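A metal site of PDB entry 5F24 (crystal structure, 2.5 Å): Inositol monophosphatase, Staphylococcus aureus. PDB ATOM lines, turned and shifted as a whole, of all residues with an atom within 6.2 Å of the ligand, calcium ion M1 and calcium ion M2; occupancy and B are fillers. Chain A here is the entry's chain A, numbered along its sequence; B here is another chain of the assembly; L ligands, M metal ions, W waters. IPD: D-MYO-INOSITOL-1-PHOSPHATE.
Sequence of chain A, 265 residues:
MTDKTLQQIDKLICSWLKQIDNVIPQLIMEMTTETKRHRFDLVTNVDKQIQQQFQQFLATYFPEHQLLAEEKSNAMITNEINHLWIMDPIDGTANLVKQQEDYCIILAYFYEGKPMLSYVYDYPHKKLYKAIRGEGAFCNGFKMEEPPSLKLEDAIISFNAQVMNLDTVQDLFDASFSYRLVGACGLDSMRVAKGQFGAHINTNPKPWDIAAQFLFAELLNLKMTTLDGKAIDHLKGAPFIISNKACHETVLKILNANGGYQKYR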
ATOM      1  N   ASP A  47      17.411  -1.943   0.801  1.00  0.00           N
ATOM      2  CA  ASP A  47      17.102  -0.593   1.281  1.00  0.00           C
ATOM      3  C   ASP A  47      18.287   0.331   1.044  1.00  0.00           C
ATOM      4  O   ASP A  47      18.122   1.412   0.477  1.00  0.00           O
ATOM      5  CB  ASP A  47      16.744  -0.602   2.772  1.00  0.00           C
ATOM      6  CG  ASP A  47      15.608  -1.562   3.117  1.00  0.00           C
ATOM      7  OD1 ASP A  47      15.713  -2.783   2.814  1.00  0.00           O
ATOM      8  OD2 ASP A  47      14.632  -1.129   3.768  1.00  0.00           O
ATOM      9  N   GLU A  70      14.961   7.226   5.419  1.00  0.00           N
ATOM     10  CA  GLU A  70      15.015   6.314   6.583  1.00  0.00           C
ATOM     11  C   GLU A  70      16.434   5.967   6.962  1.00  0.00           C
ATOM     12  O   GLU A  70      16.819   6.004   8.125  1.00  0.00           O
ATOM     13  CB  GLU A  70      14.211   5.029   6.338  1.00  0.00           C
ATOM     14  CG  GLU A  70      14.236   4.078   7.558  1.00  0.00           C
ATOM     15  CD  GLU A  70      13.127   3.043   7.512  1.00  0.00           C
ATOM     16  OE1 GLU A  70      12.964   2.336   8.513  1.00  0.00           O
ATOM     17  OE2 GLU A  70      12.438   2.967   6.471  1.00  0.00           O
ATOM     18  N   GLU A  71      17.238   5.580   5.975  1.00  0.00           N
ATOM     19  CA  GLU A  71      18.551   4.949   6.240  1.00  0.00           C
ATOM     20  C   GLU A  71      19.705   5.977   6.383  1.00  0.00           C
ATOM     21  O   GLU A  71      20.851   5.667   6.196  1.00  0.00           O
ATOM     22  CB  GLU A  71      18.924   3.917   5.139  1.00  0.00           C
ATOM     23  CG  GLU A  71      17.828   2.910   4.754  1.00  0.00           C
ATOM     24  CD  GLU A  71      17.250   2.126   5.935  1.00  0.00           C
ATOM     25  OE1 GLU A  71      18.001   1.840   6.907  1.00  0.00           O
ATOM     26  OE2 GLU A  71      16.049   1.815   5.878  1.00  0.00           O
ATOM     27  N   ASP A  88      11.265   6.620   1.420  1.00  0.00           N
ATOM     28  CA  ASP A  88      11.403   5.307   2.041  1.00  0.00           C
ATOM     29  C   ASP A  88      11.886   4.331   0.972  1.00  0.00           C
ATOM     30  O   ASP A  88      11.156   3.983   0.011  1.00  0.00           O
ATOM     31  CB  ASP A  88      10.147   4.788   2.697  1.00  0.00           C
ATOM     32  CG  ASP A  88      10.421   3.635   3.631  1.00  0.00           C
ATOM     33  OD1 ASP A  88      11.454   2.957   3.429  1.00  0.00           O
ATOM     34  OD2 ASP A  88       9.596   3.409   4.562  1.00  0.00           O
ATOM     35  N   PRO A  89      13.147   3.943   1.051  1.00  0.00           N
ATOM     36  CA  PRO A  89      13.704   3.201  -0.108  1.00  0.00           C
ATOM     37  C   PRO A  89      13.073   1.832  -0.266  1.00  0.00           C
ATOM     38  O   PRO A  89      12.910   1.389  -1.401  1.00  0.00           O
ATOM     39  CB  PRO A  89      15.198   3.111   0.210  1.00  0.00           C
ATOM     40  CG  PRO A  89      15.292   3.307   1.688  1.00  0.00           C
ATOM     41  CD  PRO A  89      14.183   4.229   2.051  1.00  0.00           C
ATOM     42  N   ILE A  90      12.766   1.154   0.821  1.00  0.00           N
ATOM     43  CA  ILE A  90      11.833   0.020   0.791  1.00  0.00           C
ATOM     44  C   ILE A  90      10.828   0.202   1.932  1.00  0.00           C
ATOM     45  O   ILE A  90      11.198   0.187   3.091  1.00  0.00           O
ATOM     46  CB  ILE A  90      12.555  -1.313   0.987  1.00  0.00           C
ATOM     47  CG1 ILE A  90      13.494  -1.575  -0.179  1.00  0.00           C
ATOM     48  CG2 ILE A  90      11.539  -2.436   1.109  1.00  0.00           C
ATOM     49  CD1 ILE A  90      12.799  -1.853  -1.505  1.00  0.00           C
ATOM     50  N   ASP A  91       9.574   0.379   1.577  1.00  0.00           N
ATOM     51  CA  ASP A  91       8.503   0.362   2.592  1.00  0.00           C
ATOM     52  C   ASP A  91       7.937  -1.013   2.527  1.00  0.00           C
ATOM     53  O   ASP A  91       7.591  -1.452   1.475  1.00  0.00           O
ATOM     54  CB  ASP A  91       7.448   1.429   2.339  1.00  0.00           C
ATOM     55  CG  ASP A  91       6.337   1.449   3.385  1.00  0.00           C
ATOM     56  OD1 ASP A  91       6.638   1.480   4.599  1.00  0.00           O
ATOM     57  OD2 ASP A  91       5.161   1.390   2.970  1.00  0.00           O
ATOM     58  N   GLY A  92       7.816  -1.686   3.641  1.00  0.00           N
ATOM     59  CA  GLY A  92       7.451  -3.122   3.668  1.00  0.00           C
ATOM     60  C   GLY A  92       8.622  -4.082   3.665  1.00  0.00           C
ATOM     61  O   GLY A  92       8.615  -5.120   2.976  1.00  0.00           O
ATOM     62  N   THR A  93       9.673  -3.723   4.383  1.00  0.00           N
ATOM     63  CA  THR A  93      10.925  -4.518   4.427  1.00  0.00           C
ATOM     64  C   THR A  93      10.609  -5.935   4.911  1.00  0.00           C
ATOM     65  O   THR A  93      11.178  -6.901   4.417  1.00  0.00           O
ATOM     66  CB  THR A  93      11.980  -3.792   5.326  1.00  0.00           C
ATOM     67  OG1 THR A  93      12.407  -2.564   4.683  1.00  0.00           O
ATOM     68  CG2 THR A  93      13.195  -4.600   5.547  1.00  0.00           C
ATOM     69  N   ALA A  94       9.697  -6.079   5.866  1.00  0.00           N
ATOM     70  CA  ALA A  94       9.321  -7.391   6.369  1.00  0.00           C
ATOM     71  C   ALA A  94       8.766  -8.235   5.236  1.00  0.00           C
ATOM     72  O   ALA A  94       9.184  -9.378   5.059  1.00  0.00           O
ATOM     73  CB  ALA A  94       8.312  -7.272   7.495  1.00  0.00           C
ATOM     74  N   ILE A 106       8.872   4.571  -1.778  1.00  0.00           N
ATOM     75  CA  ILE A 106       8.122   5.808  -1.578  1.00  0.00           C
ATOM     76  C   ILE A 106       9.036   7.056  -1.758  1.00  0.00           C
ATOM     77  O   ILE A 106      10.081   7.165  -1.139  1.00  0.00           O
ATOM     78  CB  ILE A 106       7.488   5.810  -0.175  1.00  0.00           C
ATOM     79  CG1 ILE A 106       6.597   4.587   0.041  1.00  0.00           C
ATOM     80  CG2 ILE A 106       6.617   7.042   0.030  1.00  0.00           C
ATOM     81  CD1 ILE A 106       5.923   4.520   1.394  1.00  0.00           C
ATOM     82  N   ASN A 160      -2.748  -2.218  11.715  1.00  0.00           N
ATOM     83  CA  ASN A 160      -1.996  -3.214  12.486  1.00  0.00           C
ATOM     84  C   ASN A 160      -2.758  -3.498  13.767  1.00  0.00           C
ATOM     85  O   ASN A 160      -2.802  -2.652  14.672  1.00  0.00           O
ATOM     86  CB  ASN A 160      -0.595  -2.718  12.825  1.00  0.00           C
ATOM     87  CG  ASN A 160       0.239  -3.757  13.569  1.00  0.00           C
ATOM     88  OD1 ASN A 160      -0.272  -4.779  13.983  1.00  0.00           O
ATOM     89  ND2 ASN A 160       1.531  -3.478  13.748  1.00  0.00           N
ATOM     90  N   LEU A 181      -4.978  -6.785   5.445  1.00  0.00           N
ATOM     91  CA  LEU A 181      -3.689  -6.113   5.622  1.00  0.00           C
ATOM     92  C   LEU A 181      -2.733  -6.539   4.528  1.00  0.00           C
ATOM     93  O   LEU A 181      -2.353  -7.702   4.429  1.00  0.00           O
ATOM     94  CB  LEU A 181      -3.106  -6.410   7.001  1.00  0.00           C
ATOM     95  CG  LEU A 181      -1.809  -5.672   7.373  1.00  0.00           C
ATOM     96  CD1 LEU A 181      -1.921  -4.175   7.320  1.00  0.00           C
ATOM     97  CD2 LEU A 181      -1.374  -6.077   8.769  1.00  0.00           C
ATOM     98  N   GLY A 183       0.355  -4.831   4.443  1.00  0.00           N
ATOM     99  CA  GLY A 183       1.519  -4.830   5.330  1.00  0.00           C
ATOM    100  C   GLY A 183       2.624  -3.868   4.908  1.00  0.00           C
ATOM    101  O   GLY A 183       3.762  -3.972   5.362  1.00  0.00           O
ATOM    102  N   ALA A 184       2.331  -3.011   3.961  1.00  0.00           N
ATOM    103  CA  ALA A 184       3.233  -1.894   3.662  1.00  0.00           C
ATOM    104  C   ALA A 184       2.432  -0.628   3.654  1.00  0.00           C
ATOM    105  O   ALA A 184       1.519  -0.501   2.856  1.00  0.00           O
ATOM    106  CB  ALA A 184       3.941  -2.083   2.347  1.00  0.00           C
ATOM    107  N   CYS A 185       2.782   0.343   4.498  1.00  0.00           N
ATOM    108  CA  CYS A 185       1.992   1.589   4.631  1.00  0.00           C
ATOM    109  C   CYS A 185       1.650   2.221   3.285  1.00  0.00           C
ATOM    110  O   CYS A 185       0.493   2.591   3.063  1.00  0.00           O
ATOM    111  CB  CYS A 185       2.725   2.586   5.477  1.00  0.00           C
ATOM    112  SG  CYS A 185       1.738   4.042   5.910  1.00  0.00           S
ATOM    113  N   GLY A 186       2.635   2.369   2.422  1.00  0.00           N
ATOM    114  CA  GLY A 186       2.419   2.875   1.080  1.00  0.00           C
ATOM    115  C   GLY A 186       1.382   2.107   0.274  1.00  0.00           C
ATOM    116  O   GLY A 186       0.568   2.695  -0.464  1.00  0.00           O
ATOM    117  N   ASP A 188      -1.009  -0.247   1.470  1.00  0.00           N
ATOM    118  CA  ASP A 188      -2.279  -0.161   2.136  1.00  0.00           C
ATOM    119  C   ASP A 188      -2.909   1.222   1.915  1.00  0.00           C
ATOM    120  O   ASP A 188      -4.116   1.335   1.711  1.00  0.00           O
ATOM    121  CB  ASP A 188      -2.132  -0.422   3.627  1.00  0.00           C
ATOM    122  CG  ASP A 188      -1.854  -1.890   3.951  1.00  0.00           C
ATOM    123  OD1 ASP A 188      -2.797  -2.683   3.913  1.00  0.00           O
ATOM    124  OD2 ASP A 188      -0.712  -2.243   4.304  1.00  0.00           O
ATOM    125  N   HIS A 200      -6.924   3.304   5.947  1.00  0.00           N
ATOM    126  CA  HIS A 200      -5.755   2.677   6.503  1.00  0.00           C
ATOM    127  C   HIS A 200      -5.299   3.492   7.701  1.00  0.00           C
ATOM    128  O   HIS A 200      -5.275   4.732   7.623  1.00  0.00           O
ATOM    129  CB  HIS A 200      -4.646   2.494   5.460  1.00  0.00           C
ATOM    130  CG  HIS A 200      -3.373   1.961   6.035  1.00  0.00           C
ATOM    131  ND1 HIS A 200      -3.264   0.699   6.564  1.00  0.00           N
ATOM    132  CD2 HIS A 200      -2.155   2.545   6.218  1.00  0.00           C
ATOM    133  CE1 HIS A 200      -2.034   0.506   7.025  1.00  0.00           C
ATOM    134  NE2 HIS A 200      -1.350   1.626   6.844  1.00  0.00           N
ATOM    135  N   ASN A 202      -2.156   3.978  10.657  1.00  0.00           N
ATOM    136  CA  ASN A 202      -0.865   3.649  11.232  1.00  0.00           C
ATOM    137  C   ASN A 202      -0.641   4.512  12.486  1.00  0.00           C
ATOM    138  O   ASN A 202      -0.555   5.759  12.419  1.00  0.00           O
ATOM    139  CB  ASN A 202       0.265   3.909  10.261  1.00  0.00           C
ATOM    140  CG  ASN A 202       1.618   3.423  10.791  1.00  0.00           C
ATOM    141  OD1 ASN A 202       2.009   3.731  11.920  1.00  0.00           O
ATOM    142  ND2 ASN A 202       2.343   2.675   9.976  1.00  0.00           N
ATOM    143  N   ASN A 204       1.842   4.942  14.487  1.00  0.00           N
ATOM    144  CA  ASN A 204       3.132   5.551  14.770  1.00  0.00           C
ATOM    145  C   ASN A 204       4.044   5.624  13.528  1.00  0.00           C
ATOM    146  O   ASN A 204       5.096   4.982  13.502  1.00  0.00           O
ATOM    147  CB  ASN A 204       3.834   4.721  15.836  1.00  0.00           C
ATOM    148  CG  ASN A 204       5.064   5.406  16.423  1.00  0.00           C
ATOM    149  OD1 ASN A 204       5.838   4.761  17.120  1.00  0.00           O
ATOM    150  ND2 ASN A 204       5.216   6.690  16.193  1.00  0.00           N
ATOM    151  N   PRO A 205       3.612   6.348  12.498  1.00  0.00           N
ATOM    152  CA  PRO A 205       4.447   6.423  11.286  1.00  0.00           C
ATOM    153  C   PRO A 205       5.594   7.403  11.342  1.00  0.00           C
ATOM    154  O   PRO A 205       5.514   8.390  12.016  1.00  0.00           O
ATOM    155  CB  PRO A 205       3.451   6.927  10.254  1.00  0.00           C
ATOM    156  CG  PRO A 205       2.563   7.835  11.045  1.00  0.00           C
ATOM    157  CD  PRO A 205       2.400   7.173  12.386  1.00  0.00           C
ATOM    158  N   TRP A 208       8.671   9.363   6.383  1.00  0.00           N
ATOM    159  CA  TRP A 208       8.835   8.626   5.101  1.00  0.00           C
ATOM    160  C   TRP A 208       7.731   7.636   4.827  1.00  0.00           C
ATOM    161  O   TRP A 208       7.467   7.341   3.672  1.00  0.00           O
ATOM    162  CB  TRP A 208      10.210   8.012   4.932  1.00  0.00           C
ATOM    163  CG  TRP A 208      10.726   7.393   6.144  1.00  0.00           C
ATOM    164  CD1 TRP A 208      10.477   6.142   6.585  1.00  0.00           C
ATOM    165  CD2 TRP A 208      11.608   7.989   7.086  1.00  0.00           C
ATOM    166  NE1 TRP A 208      11.125   5.919   7.758  1.00  0.00           N
ATOM    167  CE2 TRP A 208      11.809   7.035   8.103  1.00  0.00           C
ATOM    168  CE3 TRP A 208      12.214   9.241   7.197  1.00  0.00           C
ATOM    169  CZ2 TRP A 208      12.629   7.293   9.213  1.00  0.00           C
ATOM    170  CZ3 TRP A 208      13.036   9.500   8.316  1.00  0.00           C
ATOM    171  CH2 TRP A 208      13.236   8.524   9.305  1.00  0.00           C
ATOM    172  N   ASP A 209       7.086   7.095   5.854  1.00  0.00           N
ATOM    173  CA  ASP A 209       5.948   6.169   5.680  1.00  0.00           C
ATOM    174  C   ASP A 209       4.728   6.806   5.059  1.00  0.00           C
ATOM    175  O   ASP A 209       3.896   6.115   4.412  1.00  0.00           O
ATOM    176  CB  ASP A 209       5.430   5.729   7.056  1.00  0.00           C
ATOM    177  CG  ASP A 209       6.331   4.745   7.746  1.00  0.00           C
ATOM    178  OD1 ASP A 209       6.814   3.808   7.089  1.00  0.00           O
ATOM    179  OD2 ASP A 209       6.556   4.929   8.967  1.00  0.00           O
ATOM    180  N   ARG B 180      -0.635 -11.265   8.393  1.00  0.00           N
ATOM    181  CA  ARG B 180      -1.169 -10.678   7.165  1.00  0.00           C
ATOM    182  C   ARG B 180      -2.410 -11.401   6.774  1.00  0.00           C
ATOM    183  O   ARG B 180      -2.674 -12.501   7.225  1.00  0.00           O
ATOM    184  CB  ARG B 180      -0.259 -10.687   5.920  1.00  0.00           C
ATOM    185  CG  ARG B 180       1.205 -10.301   6.029  1.00  0.00           C
ATOM    186  CD  ARG B 180       1.554  -8.845   5.750  1.00  0.00           C
ATOM    187  NE  ARG B 180       1.872  -8.311   7.050  1.00  0.00           N
ATOM    188  CZ  ARG B 180       3.024  -7.839   7.483  1.00  0.00           C
ATOM    189  NH1 ARG B 180       4.090  -7.653   6.728  1.00  0.00           N
ATOM    190  NH2 ARG B 180       3.063  -7.504   8.734  1.00  0.00           N
HETATM  191  C1  IPD L   1       6.917  -0.279   7.951  1.00  0.00           C
HETATM  192  C2  IPD L   1       5.747  -0.695   7.060  1.00  0.00           C
HETATM  193  C3  IPD L   1       4.726  -1.466   7.890  1.00  0.00           C
HETATM  194  C4  IPD L   1       4.450  -0.983   9.339  1.00  0.00           C
HETATM  195  C5  IPD L   1       5.394   0.043   9.964  1.00  0.00           C
HETATM  196  C6  IPD L   1       6.440   0.658   9.033  1.00  0.00           C
HETATM  197  P1  IPD L   1       9.321  -0.427   6.755  1.00  0.00           P
HETATM  198  O1  IPD L   1       7.955   0.359   7.211  1.00  0.00           O
HETATM  199  O2  IPD L   1       5.173   0.396   6.330  1.00  0.00           O
HETATM  200  O3  IPD L   1       3.509  -1.763   7.197  1.00  0.00           O
HETATM  201  O4  IPD L   1       3.076  -0.657   9.583  1.00  0.00           O
HETATM  202  O5  IPD L   1       4.632   1.065  10.578  1.00  0.00           O
HETATM  203  O6  IPD L   1       7.536   0.962   9.892  1.00  0.00           O
HETATM  204  O7  IPD L   1       8.791  -1.632   6.044  1.00  0.00           O
HETATM  205  O8  IPD L   1       9.941   0.691   5.945  1.00  0.00           O
HETATM  206  O9  IPD L   1      10.023  -0.818   8.036  1.00  0.00           O
HETATM  207 CA    CA M   1       8.244   2.323   6.077  1.00  0.00          CA
HETATM  208 CA    CA M   2      11.947   1.288   4.977  1.00  0.00          CA
HETATM  209  O   HOH W   1      14.057   1.072   4.177  1.00  0.00           O
HETATM  210  O   HOH W   2       0.732  -1.454   6.727  1.00  0.00           O
HETATM  211  O   HOH W   3       9.750   2.946   7.758  1.00  0.00           O
HETATM  212  O   HOH W   4       8.295   3.239  10.098  1.00  0.00           O
HETATM  213  O   HOH W   5       0.855  -2.309   9.283  1.00  0.00           O
HETATM  214  O   HOH W   6       1.062   1.123   7.912  1.00  0.00           O
HETATM  215  O   HOH W   7      12.265  -0.545   6.358  1.00  0.00           O
HETATM  216  O   HOH W   8       7.924  -3.878   7.031  1.00  0.00           O
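Along chain A the residues within 4 Å of calcium ion M1 span positions 88 to 209.
The nearest printed residue that does not touch calcium ion M1 is Glu 70 (4.3 Å).
Calcium ion M1 is bound by an oxygen (O1) of the ligand (2.3 Å), the side-chain carboxylate of Asp 209 (2.3 Å), the side-chain carboxylate of Asp 88 (2.3 Å), the side-chain carboxylate of Asp 91 (2.3 Å), water W3 (2.3 Å) and an oxygen (O8) of the ligand (2.4 Å).
Calcium ion M1 has six donor atoms within binding distance.
OE2 of Glu 70 lies close to NE1 of Trp 208 (3.5 Å).
N of Asp 88 is in hydrogen-bond range of O of Ile 106, at 2.9 Å.
N of Cys 185 sits at hydrogen-bond distance from OD2 of Asp 91 (3.0 Å).
The side-chain carboxylate (OD2) of Asp 91 sits at hydrogen-bond distance from the backbone NH (N) of Gly 186 (2.8 Å).
OG1 of Thr 93 lies within hydrogen-bond range of OD2 of Asp 47 (2.8 Å).
The side-chain amide oxygen (OD1) of Asn 202 lies within hydrogen-bond range of the backbone NH (N) of Asn 204, 2.8 Å away.
N of Gly 183 lies within hydrogen-bond range of OD2 of Asp 188 (2.8 Å).
The side-chain carboxylate (OD2) of Asp 188 sits at hydrogen-bond distance from the backbone NH (N) of Ala 184.
Merely in contact with the ligand: Ala 184 (3.5 Å).
11 residues have an atom within 4 Å of the ligand: Glu 70, Asp 88, Ile 90, Asp 91, Gly 92, Thr 93, Gly 183, Ala 184, Cys 185, Asn 202 and Asp 209.
The nearest printed residue that does not touch the ligand is Ala 94 (4.5 Å).
Water W3 lies within hydrogen-bond range of the indole nitrogen (NE1) of Trp 208 (3.3 Å) and the side-chain carboxylate (OE1) of Glu 70 (3.4 Å).
Water W7 bridges OG1 of Thr 93 (2.6 Å) and O9 of the ligand (2.8 Å).
Water W4 bridges an oxygen (O6) of the ligand (2.4 Å) and the side-chain carboxylate (OD2) of Asp 209 (2.7 Å).
Water W8 lies within hydrogen-bond range of O7 of the ligand (2.6 Å), N of Ala 94 (3.1 Å) and N of Thr 93 (3.2 Å).
Water W2 lies within hydrogen-bond range of an oxygen (O3) of the ligand (2.8 Å) and the side-chain carboxylate (OD2) of Asp 188 (2.9 Å).
Water W6 lies within hydrogen-bond range of a ring nitrogen (NE2) of His 200 (2.7 Å), the side-chain amide nitrogen of Asn 202 (2.9 Å), an oxygen (O4) of the ligand (3.2 Å) and the side-chain sulfur of Cys 185 (3.6 Å).
Calcium ion M2 is bound by water W1 (2.3 Å), the side-chain carboxylate of Glu 70 (2.3 Å), an oxygen (O8) of the ligand (2.3 Å), the backbone carbonyl oxygen of Ile 90 (2.3 Å), water W7 (2.3 Å) and the side-chain carboxylate of Asp 88 (2.3 Å).
An oxygen (O7) of the ligand lies within hydrogen-bond range of the backbone NH (N) of Gly 92 (2.6 Å).
The backbone NH (N) of Thr 93 lies within hydrogen-bond range of an oxygen (O7) of the ligand (2.8 Å).
The side-chain amide nitrogen (ND2) of Asn 202 sits at hydrogen-bond distance from an oxygen (O5) of the ligand, at 2.9 Å.
O of Gly 183 sits at hydrogen-bond distance from O3 of the ligand.
N of Cys 185 sits at hydrogen-bond distance from O2 of the ligand (3.0 Å).
Asp 47 touches calcium ion M2.
Thr 93 touches calcium ion M2 (OG1 to CA, 3.9 Å).
Within 4 Å of calcium ion M2: Asp 47, Glu 70, Asp 88, Ile 90 and Thr 93.
The nearest printed residue that does not touch calcium ion M2 is Glu 71 (4.2 Å).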
